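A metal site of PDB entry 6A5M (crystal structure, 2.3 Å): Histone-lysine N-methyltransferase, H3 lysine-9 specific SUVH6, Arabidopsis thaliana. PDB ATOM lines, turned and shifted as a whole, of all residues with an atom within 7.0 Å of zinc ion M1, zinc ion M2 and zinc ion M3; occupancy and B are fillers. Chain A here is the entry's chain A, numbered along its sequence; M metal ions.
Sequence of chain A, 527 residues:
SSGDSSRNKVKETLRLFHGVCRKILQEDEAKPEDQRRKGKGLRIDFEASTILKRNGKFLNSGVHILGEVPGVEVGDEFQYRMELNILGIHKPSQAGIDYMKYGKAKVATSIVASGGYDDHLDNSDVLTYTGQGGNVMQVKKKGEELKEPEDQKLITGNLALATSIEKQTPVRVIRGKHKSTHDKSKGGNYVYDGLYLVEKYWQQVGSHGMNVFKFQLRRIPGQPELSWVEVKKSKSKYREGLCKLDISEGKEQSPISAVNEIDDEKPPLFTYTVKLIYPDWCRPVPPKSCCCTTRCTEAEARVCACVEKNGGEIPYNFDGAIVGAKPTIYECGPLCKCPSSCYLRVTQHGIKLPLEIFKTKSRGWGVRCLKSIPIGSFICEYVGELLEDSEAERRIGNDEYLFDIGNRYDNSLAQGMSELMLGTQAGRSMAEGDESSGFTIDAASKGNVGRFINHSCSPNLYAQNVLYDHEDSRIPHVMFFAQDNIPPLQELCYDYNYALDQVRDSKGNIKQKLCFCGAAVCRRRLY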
ATOM      1  N   LYS A 288     -20.849 -34.926   2.426  1.00  0.00           N
ATOM      2  CA  LYS A 288     -19.582 -35.511   2.836  1.00  0.00           C
ATOM      3  C   LYS A 288     -18.567 -34.407   3.012  1.00  0.00           C
ATOM      4  O   LYS A 288     -18.414 -33.544   2.158  1.00  0.00           O
ATOM      5  CB  LYS A 288     -19.086 -36.555   1.811  1.00  0.00           C
ATOM      6  CG  LYS A 288     -20.186 -37.497   1.237  1.00  0.00           C
ATOM      7  CD  LYS A 288     -21.282 -37.946   2.219  1.00  0.00           C
ATOM      8  CE  LYS A 288     -20.770 -38.383   3.591  1.00  0.00           C
ATOM      9  NZ  LYS A 288     -21.844 -38.228   4.607  1.00  0.00           N
ATOM     10  N   SER A 289     -17.966 -34.456   4.204  1.00  0.00           N
ATOM     11  CA  SER A 289     -17.237 -33.385   4.837  1.00  0.00           C
ATOM     12  C   SER A 289     -15.763 -33.354   4.494  1.00  0.00           C
ATOM     13  O   SER A 289     -15.301 -34.018   3.557  1.00  0.00           O
ATOM     14  CB  SER A 289     -17.401 -33.452   6.358  1.00  0.00           C
ATOM     15  OG  SER A 289     -16.432 -34.295   6.947  1.00  0.00           O
ATOM     16  N   CYS A 290     -15.019 -32.592   5.283  1.00  0.00           N
ATOM     17  CA  CYS A 290     -13.643 -32.258   4.971  1.00  0.00           C
ATOM     18  C   CYS A 290     -12.686 -32.553   6.107  1.00  0.00           C
ATOM     19  O   CYS A 290     -13.057 -32.512   7.279  1.00  0.00           O
ATOM     20  CB  CYS A 290     -13.560 -30.794   4.590  1.00  0.00           C
ATOM     21  SG  CYS A 290     -12.091 -30.403   3.639  1.00  0.00           S
ATOM     22  N   CYS A 291     -11.439 -32.840   5.751  1.00  0.00           N
ATOM     23  CA  CYS A 291     -10.412 -33.150   6.738  1.00  0.00           C
ATOM     24  C   CYS A 291      -9.201 -32.252   6.512  1.00  0.00           C
ATOM     25  O   CYS A 291      -8.151 -32.694   6.043  1.00  0.00           O
ATOM     26  CB  CYS A 291     -10.007 -34.615   6.642  1.00  0.00           C
ATOM     27  SG  CYS A 291     -10.999 -35.733   7.668  1.00  0.00           S
ATOM     28  N   CYS A 292      -9.359 -30.982   6.863  1.00  0.00           N
ATOM     29  CA  CYS A 292      -8.307 -29.981   6.763  1.00  0.00           C
ATOM     30  C   CYS A 292      -8.544 -29.004   7.905  1.00  0.00           C
ATOM     31  O   CYS A 292      -9.642 -28.501   8.079  1.00  0.00           O
ATOM     32  CB  CYS A 292      -8.347 -29.269   5.401  1.00  0.00           C
ATOM     33  SG  CYS A 292      -8.481 -30.343   3.929  1.00  0.00           S
ATOM     34  N   THR A 293      -7.508 -28.760   8.703  1.00  0.00           N
ATOM     35  CA  THR A 293      -7.659 -27.892   9.865  1.00  0.00           C
ATOM     36  C   THR A 293      -7.463 -26.426   9.509  1.00  0.00           C
ATOM     37  O   THR A 293      -7.688 -25.539  10.323  1.00  0.00           O
ATOM     38  CB  THR A 293      -6.702 -28.266  10.984  1.00  0.00           C
ATOM     39  OG1 THR A 293      -7.027 -27.520  12.164  1.00  0.00           O
ATOM     40  CG2 THR A 293      -5.266 -27.966  10.571  1.00  0.00           C
ATOM     41  N   THR A 294      -7.011 -26.179   8.282  1.00  0.00           N
ATOM     42  CA  THR A 294      -6.835 -24.821   7.823  1.00  0.00           C
ATOM     43  C   THR A 294      -7.411 -24.642   6.428  1.00  0.00           C
ATOM     44  O   THR A 294      -8.030 -25.562   5.895  1.00  0.00           O
ATOM     45  CB  THR A 294      -5.374 -24.426   7.812  1.00  0.00           C
ATOM     46  OG1 THR A 294      -5.275 -23.050   7.445  1.00  0.00           O
ATOM     47  CG2 THR A 294      -4.607 -25.283   6.802  1.00  0.00           C
ATOM     48  N   ARG A 295      -7.199 -23.471   5.830  1.00  0.00           N
ATOM     49  CA  ARG A 295      -7.722 -23.194   4.489  1.00  0.00           C
ATOM     50  C   ARG A 295      -7.368 -24.289   3.497  1.00  0.00           C
ATOM     51  O   ARG A 295      -6.207 -24.673   3.376  1.00  0.00           O
ATOM     52  CB  ARG A 295      -7.209 -21.852   3.946  1.00  0.00           C
ATOM     53  CG  ARG A 295      -7.347 -20.664   4.874  1.00  0.00           C
ATOM     54  CD  ARG A 295      -6.890 -19.414   4.157  1.00  0.00           C
ATOM     55  NE  ARG A 295      -7.157 -18.200   4.917  1.00  0.00           N
ATOM     56  CZ  ARG A 295      -7.121 -16.970   4.412  1.00  0.00           C
ATOM     57  NH1 ARG A 295      -7.366 -15.931   5.179  1.00  0.00           N
ATOM     58  NH2 ARG A 295      -6.833 -16.793   3.129  1.00  0.00           N
ATOM     59  N   CYS A 296      -8.376 -24.786   2.792  1.00  0.00           N
ATOM     60  CA  CYS A 296      -8.159 -25.827   1.791  1.00  0.00           C
ATOM     61  C   CYS A 296      -7.483 -25.265   0.567  1.00  0.00           C
ATOM     62  O   CYS A 296      -7.855 -24.203   0.063  1.00  0.00           O
ATOM     63  CB  CYS A 296      -9.459 -26.491   1.382  1.00  0.00           C
ATOM     64  SG  CYS A 296     -10.244 -27.312   2.735  1.00  0.00           S
ATOM     65  N   THR A 297      -6.465 -25.994   0.139  1.00  0.00           N
ATOM     66  CA  THR A 297      -5.706 -25.702  -1.037  1.00  0.00           C
ATOM     67  C   THR A 297      -5.130 -26.977  -1.649  1.00  0.00           C
ATOM     68  O   THR A 297      -4.906 -27.935  -0.953  1.00  0.00           O
ATOM     69  CB  THR A 297      -4.613 -24.684  -0.726  1.00  0.00           C
ATOM     70  OG1 THR A 297      -3.591 -24.742  -1.716  1.00  0.00           O
ATOM     71  CG2 THR A 297      -3.983 -24.956   0.582  1.00  0.00           C
ATOM     72  N   VAL A 303      -5.078 -35.270   1.658  1.00  0.00           N
ATOM     73  CA  VAL A 303      -6.298 -35.263   0.861  1.00  0.00           C
ATOM     74  C   VAL A 303      -7.352 -34.270   1.338  1.00  0.00           C
ATOM     75  O   VAL A 303      -7.698 -34.252   2.494  1.00  0.00           O
ATOM     76  CB  VAL A 303      -6.926 -36.674   0.825  1.00  0.00           C
ATOM     77  CG1 VAL A 303      -8.287 -36.675   0.127  1.00  0.00           C
ATOM     78  CG2 VAL A 303      -6.007 -37.638   0.122  1.00  0.00           C
ATOM     79  N   CYS A 304      -7.897 -33.498   0.415  1.00  0.00           N
ATOM     80  CA  CYS A 304      -9.105 -32.735   0.690  1.00  0.00           C
ATOM     81  C   CYS A 304     -10.224 -33.219  -0.236  1.00  0.00           C
ATOM     82  O   CYS A 304     -10.150 -33.049  -1.453  1.00  0.00           O
ATOM     83  CB  CYS A 304      -8.882 -31.227   0.495  1.00  0.00           C
ATOM     84  SG  CYS A 304     -10.397 -30.247   0.681  1.00  0.00           S
ATOM     85  N   ALA A 305     -11.242 -33.842   0.357  1.00  0.00           N
ATOM     86  CA  ALA A 305     -12.364 -34.409  -0.394  1.00  0.00           C
ATOM     87  C   ALA A 305     -13.081 -33.357  -1.227  1.00  0.00           C
ATOM     88  O   ALA A 305     -13.546 -33.623  -2.335  1.00  0.00           O
ATOM     89  CB  ALA A 305     -13.347 -35.054   0.557  1.00  0.00           C
ATOM     90  N   CYS A 306     -13.168 -32.147  -0.689  1.00  0.00           N
ATOM     91  CA  CYS A 306     -13.895 -31.089  -1.365  1.00  0.00           C
ATOM     92  C   CYS A 306     -13.159 -30.623  -2.619  1.00  0.00           C
ATOM     93  O   CYS A 306     -13.790 -30.239  -3.601  1.00  0.00           O
ATOM     94  CB  CYS A 306     -14.152 -29.943  -0.383  1.00  0.00           C
ATOM     95  SG  CYS A 306     -15.122 -30.518   1.057  1.00  0.00           S
ATOM     96  N   VAL A 307     -11.830 -30.696  -2.623  1.00  0.00           N
ATOM     97  CA  VAL A 307     -11.056 -30.423  -3.836  1.00  0.00           C
ATOM     98  C   VAL A 307     -11.278 -31.500  -4.906  1.00  0.00           C
ATOM     99  O   VAL A 307     -11.283 -31.198  -6.108  1.00  0.00           O
ATOM    100  CB  VAL A 307      -9.543 -30.312  -3.530  1.00  0.00           C
ATOM    101  CG1 VAL A 307      -8.728 -30.171  -4.809  1.00  0.00           C
ATOM    102  CG2 VAL A 307      -9.280 -29.152  -2.584  1.00  0.00           C
ATOM    103  N   LYS A 309     -14.076 -33.196  -5.163  1.00  0.00           N
ATOM    104  CA  LYS A 309     -15.432 -32.930  -5.645  1.00  0.00           C
ATOM    105  C   LYS A 309     -15.400 -31.964  -6.831  1.00  0.00           C
ATOM    106  O   LYS A 309     -16.194 -32.079  -7.755  1.00  0.00           O
ATOM    107  CB  LYS A 309     -16.304 -32.341  -4.540  1.00  0.00           C
ATOM    108  CG  LYS A 309     -16.887 -33.352  -3.575  1.00  0.00           C
ATOM    109  CD  LYS A 309     -17.667 -32.626  -2.474  1.00  0.00           C
ATOM    110  CE  LYS A 309     -17.860 -33.528  -1.252  1.00  0.00           C
ATOM    111  NZ  LYS A 309     -18.466 -32.780  -0.118  1.00  0.00           N
ATOM    112  N   GLU A 331     -18.487 -26.108  -2.475  1.00  0.00           N
ATOM    113  CA  GLU A 331     -17.817 -25.385  -1.408  1.00  0.00           C
ATOM    114  C   GLU A 331     -17.746 -26.264  -0.154  1.00  0.00           C
ATOM    115  O   GLU A 331     -18.490 -27.243  -0.043  1.00  0.00           O
ATOM    116  CB  GLU A 331     -18.541 -24.063  -1.094  1.00  0.00           C
ATOM    117  CG  GLU A 331     -18.228 -22.917  -2.090  1.00  0.00           C
ATOM    118  CD  GLU A 331     -18.891 -21.595  -1.700  1.00  0.00           C
ATOM    119  OE1 GLU A 331     -19.215 -21.416  -0.509  1.00  0.00           O
ATOM    120  OE2 GLU A 331     -19.095 -20.731  -2.572  1.00  0.00           O
ATOM    121  N   CYS A 332     -16.866 -25.926   0.772  1.00  0.00           N
ATOM    122  CA  CYS A 332     -16.800 -26.647   2.030  1.00  0.00           C
ATOM    123  C   CYS A 332     -18.062 -26.363   2.822  1.00  0.00           C
ATOM    124  O   CYS A 332     -18.624 -25.271   2.736  1.00  0.00           O
ATOM    125  CB  CYS A 332     -15.551 -26.255   2.840  1.00  0.00           C
ATOM    126  SG  CYS A 332     -14.043 -26.954   2.137  1.00  0.00           S
ATOM    127  N   GLY A 333     -18.516 -27.370   3.576  1.00  0.00           N
ATOM    128  CA  GLY A 333     -19.821 -27.322   4.207  1.00  0.00           C
ATOM    129  C   GLY A 333     -19.741 -27.141   5.710  1.00  0.00           C
ATOM    130  O   GLY A 333     -18.703 -26.739   6.235  1.00  0.00           O
ATOM    131  N   LEU A 335     -19.761 -29.230   8.203  1.00  0.00           N
ATOM    132  CA  LEU A 335     -18.991 -30.176   8.981  1.00  0.00           C
ATOM    133  C   LEU A 335     -17.559 -30.324   8.453  1.00  0.00           C
ATOM    134  O   LEU A 335     -16.848 -31.226   8.889  1.00  0.00           O
ATOM    135  CB  LEU A 335     -19.681 -31.540   9.019  1.00  0.00           C
ATOM    136  CG  LEU A 335     -21.053 -31.569   9.700  1.00  0.00           C
ATOM    137  CD1 LEU A 335     -21.510 -32.996   9.915  1.00  0.00           C
ATOM    138  CD2 LEU A 335     -21.025 -30.814  11.003  1.00  0.00           C
ATOM    139  N   CYS A 336     -17.141 -29.471   7.525  1.00  0.00           N
ATOM    140  CA  CYS A 336     -15.711 -29.366   7.200  1.00  0.00           C
ATOM    141  C   CYS A 336     -14.980 -28.643   8.343  1.00  0.00           C
ATOM    142  O   CYS A 336     -15.473 -27.624   8.842  1.00  0.00           O
ATOM    143  CB  CYS A 336     -15.490 -28.643   5.866  1.00  0.00           C
ATOM    144  SG  CYS A 336     -16.157 -29.475   4.411  1.00  0.00           S
ATOM    145  N   LYS A 337     -13.831 -29.147   8.759  1.00  0.00           N
ATOM    146  CA  LYS A 337     -13.106 -28.563   9.898  1.00  0.00           C
ATOM    147  C   LYS A 337     -12.332 -27.294   9.520  1.00  0.00           C
ATOM    148  O   LYS A 337     -11.616 -26.708  10.330  1.00  0.00           O
ATOM    149  CB  LYS A 337     -12.180 -29.607  10.502  1.00  0.00           C
ATOM    150  CG  LYS A 337     -12.868 -30.950  10.744  1.00  0.00           C
ATOM    151  CD  LYS A 337     -11.885 -32.019  11.174  1.00  0.00           C
ATOM    152  CE  LYS A 337     -12.585 -33.309  11.522  1.00  0.00           C
ATOM    153  NZ  LYS A 337     -11.629 -34.452  11.590  1.00  0.00           N
ATOM    154  N   CYS A 338     -12.552 -26.861   8.284  1.00  0.00           N
ATOM    155  CA  CYS A 338     -11.952 -25.630   7.785  1.00  0.00           C
ATOM    156  C   CYS A 338     -12.450 -24.415   8.510  1.00  0.00           C
ATOM    157  O   CYS A 338     -13.591 -24.351   8.954  1.00  0.00           O
ATOM    158  CB  CYS A 338     -12.279 -25.445   6.306  1.00  0.00           C
ATOM    159  SG  CYS A 338     -11.826 -26.861   5.326  1.00  0.00           S
ATOM    160  N   PRO A 339     -11.571 -23.430   8.600  1.00  0.00           N
ATOM    161  CA  PRO A 339     -11.949 -22.122   9.133  1.00  0.00           C
ATOM    162  C   PRO A 339     -12.847 -21.397   8.136  1.00  0.00           C
ATOM    163  O   PRO A 339     -12.914 -21.795   6.980  1.00  0.00           O
ATOM    164  CB  PRO A 339     -10.611 -21.411   9.303  1.00  0.00           C
ATOM    165  CG  PRO A 339      -9.766 -22.002   8.236  1.00  0.00           C
ATOM    166  CD  PRO A 339     -10.169 -23.449   8.158  1.00  0.00           C
ATOM    167  N   CYS A 342     -11.446 -20.397   4.619  1.00  0.00           N
ATOM    168  CA  CYS A 342     -11.073 -21.388   3.613  1.00  0.00           C
ATOM    169  C   CYS A 342     -11.370 -20.873   2.197  1.00  0.00           C
ATOM    170  O   CYS A 342     -12.359 -20.162   1.976  1.00  0.00           O
ATOM    171  CB  CYS A 342     -11.808 -22.707   3.848  1.00  0.00           C
ATOM    172  SG  CYS A 342     -11.579 -23.921   2.526  1.00  0.00           S
ATOM    173  N   TYR A 343     -10.504 -21.235   1.247  1.00  0.00           N
ATOM    174  CA  TYR A 343     -10.623 -20.727  -0.128  1.00  0.00           C
ATOM    175  C   TYR A 343     -11.841 -21.317  -0.844  1.00  0.00           C
ATOM    176  O   TYR A 343     -12.282 -20.798  -1.880  1.00  0.00           O
ATOM    177  CB  TYR A 343      -9.354 -21.033  -0.927  1.00  0.00           C
ATOM    178  CG  TYR A 343      -8.094 -20.348  -0.399  1.00  0.00           C
ATOM    179  CD1 TYR A 343      -8.030 -18.959  -0.302  1.00  0.00           C
ATOM    180  CD2 TYR A 343      -6.985 -21.091  -0.026  1.00  0.00           C
ATOM    181  CE1 TYR A 343      -6.886 -18.326   0.176  1.00  0.00           C
ATOM    182  CE2 TYR A 343      -5.832 -20.468   0.450  1.00  0.00           C
ATOM    183  CZ  TYR A 343      -5.789 -19.082   0.548  1.00  0.00           C
ATOM    184  OH  TYR A 343      -4.655 -18.456   1.008  1.00  0.00           O
ATOM    185  N   LEU A 344     -12.352 -22.413  -0.288  1.00  0.00           N
ATOM    186  CA  LEU A 344     -13.543 -23.071  -0.791  1.00  0.00           C
ATOM    187  C   LEU A 344     -14.775 -22.596  -0.039  1.00  0.00           C
ATOM    188  O   LEU A 344     -15.796 -23.255  -0.072  1.00  0.00           O
ATOM    189  CB  LEU A 344     -13.423 -24.593  -0.648  1.00  0.00           C
ATOM    190  CG  LEU A 344     -12.601 -25.323  -1.710  1.00  0.00           C
ATOM    191  CD1 LEU A 344     -13.018 -26.773  -1.792  1.00  0.00           C
ATOM    192  CD2 LEU A 344     -12.807 -24.645  -3.045  1.00  0.00           C
ATOM    193  N   ARG A 345     -14.662 -21.480   0.657  1.00  0.00           N
ATOM    194  CA  ARG A 345     -15.824 -20.897   1.321  1.00  0.00           C
ATOM    195  C   ARG A 345     -16.018 -19.475   0.815  1.00  0.00           C
ATOM    196  O   ARG A 345     -15.320 -18.561   1.261  1.00  0.00           O
ATOM    197  CB  ARG A 345     -15.671 -20.901   2.845  1.00  0.00           C
ATOM    198  CG  ARG A 345     -15.646 -22.275   3.503  1.00  0.00           C
ATOM    199  CD  ARG A 345     -15.601 -22.100   5.003  1.00  0.00           C
ATOM    200  NE  ARG A 345     -15.348 -23.317   5.770  1.00  0.00           N
ATOM    201  CZ  ARG A 345     -16.300 -24.152   6.194  1.00  0.00           C
ATOM    202  NH1 ARG A 345     -17.582 -23.933   5.906  1.00  0.00           N
ATOM    203  NH2 ARG A 345     -15.949 -25.227   6.904  1.00  0.00           N
HETATM  204 ZN    ZN M   1     -12.289 -26.003   3.319  1.00  0.00          ZN
HETATM  205 ZN    ZN M   2     -14.351 -29.276   2.873  1.00  0.00          ZN
HETATM  206 ZN    ZN M   3     -10.396 -29.438   2.748  1.00  0.00          ZN
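Within 4 Å of zinc ion M1: Cys 296, Cys 332, Cys 338 and Cys 342.
Four residues have an atom within 4 Å of zinc ion M2: Cys 290, Cys 306, Cys 332 and Cys 336. The nearest printed residue that does not touch zinc ion M2 is Cys 338 (4.3 Å).
The backbone carbonyl oxygen (O) of Cys 336 lies within hydrogen-bond range of the guanidinium group (NH2) of Arg 345 (3.1 Å). The backbone NH of Cys 338 sits at hydrogen-bond distance from the backbone carbonyl oxygen of Cys 292. The backbone NH (N) of Cys 332 sits at hydrogen-bond distance from the backbone carbonyl oxygen (O) of Leu 344 (3.0 Å). The backbone NH (N) of Leu 344 lies close to the side-chain sulfur (SG) of Cys 342, 3.3 Å away. The backbone carbonyl oxygen of Cys 338 is in hydrogen-bond range of the guanidinium group of Arg 345 (3.2 Å). The side-chain sulfur of Cys 336 sits close to the backbone NH of Gly 333. The backbone NH of Cys 306 sits close to the side-chain sulfur of Cys 304 (3.6 Å). SG of Cys 304 sits close to N of Val 307 (3.6 Å).
Zinc ion M3 is bound by the side-chain sulfur of Cys 296 (2.1 Å), the side-chain sulfur of Cys 290 (2.1 Å), the side-chain sulfur of Cys 304 (2.2 Å) and the side-chain sulfur of Cys 292 (2.4 Å). Zinc ion M3 has four donor atoms within binding distance.
The side-chain sulfur (SG) of Cys 338 is bound to zinc ion M1, 2.2 Å away. Zinc ion M1 is bound by SG of Cys 332 (2.3 Å). The side-chain sulfur (SG) of Cys 342 is bound to zinc ion M1 (2.3 Å). SG of Cys 296 is bound to zinc ion M1, at 2.5 Å.
Of the 28 residues printed, 5 come within 4 Å of zinc ion M3.
Zinc ion M2 is bound by the side-chain sulfur of Cys 306 (2.3 Å), the side-chain sulfur of Cys 336 (2.4 Å), the side-chain sulfur of Cys 332 (2.5 Å) and the side-chain sulfur of Cys 290 (2.6 Å). Zinc ion M2 has four donor atoms within binding distance.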
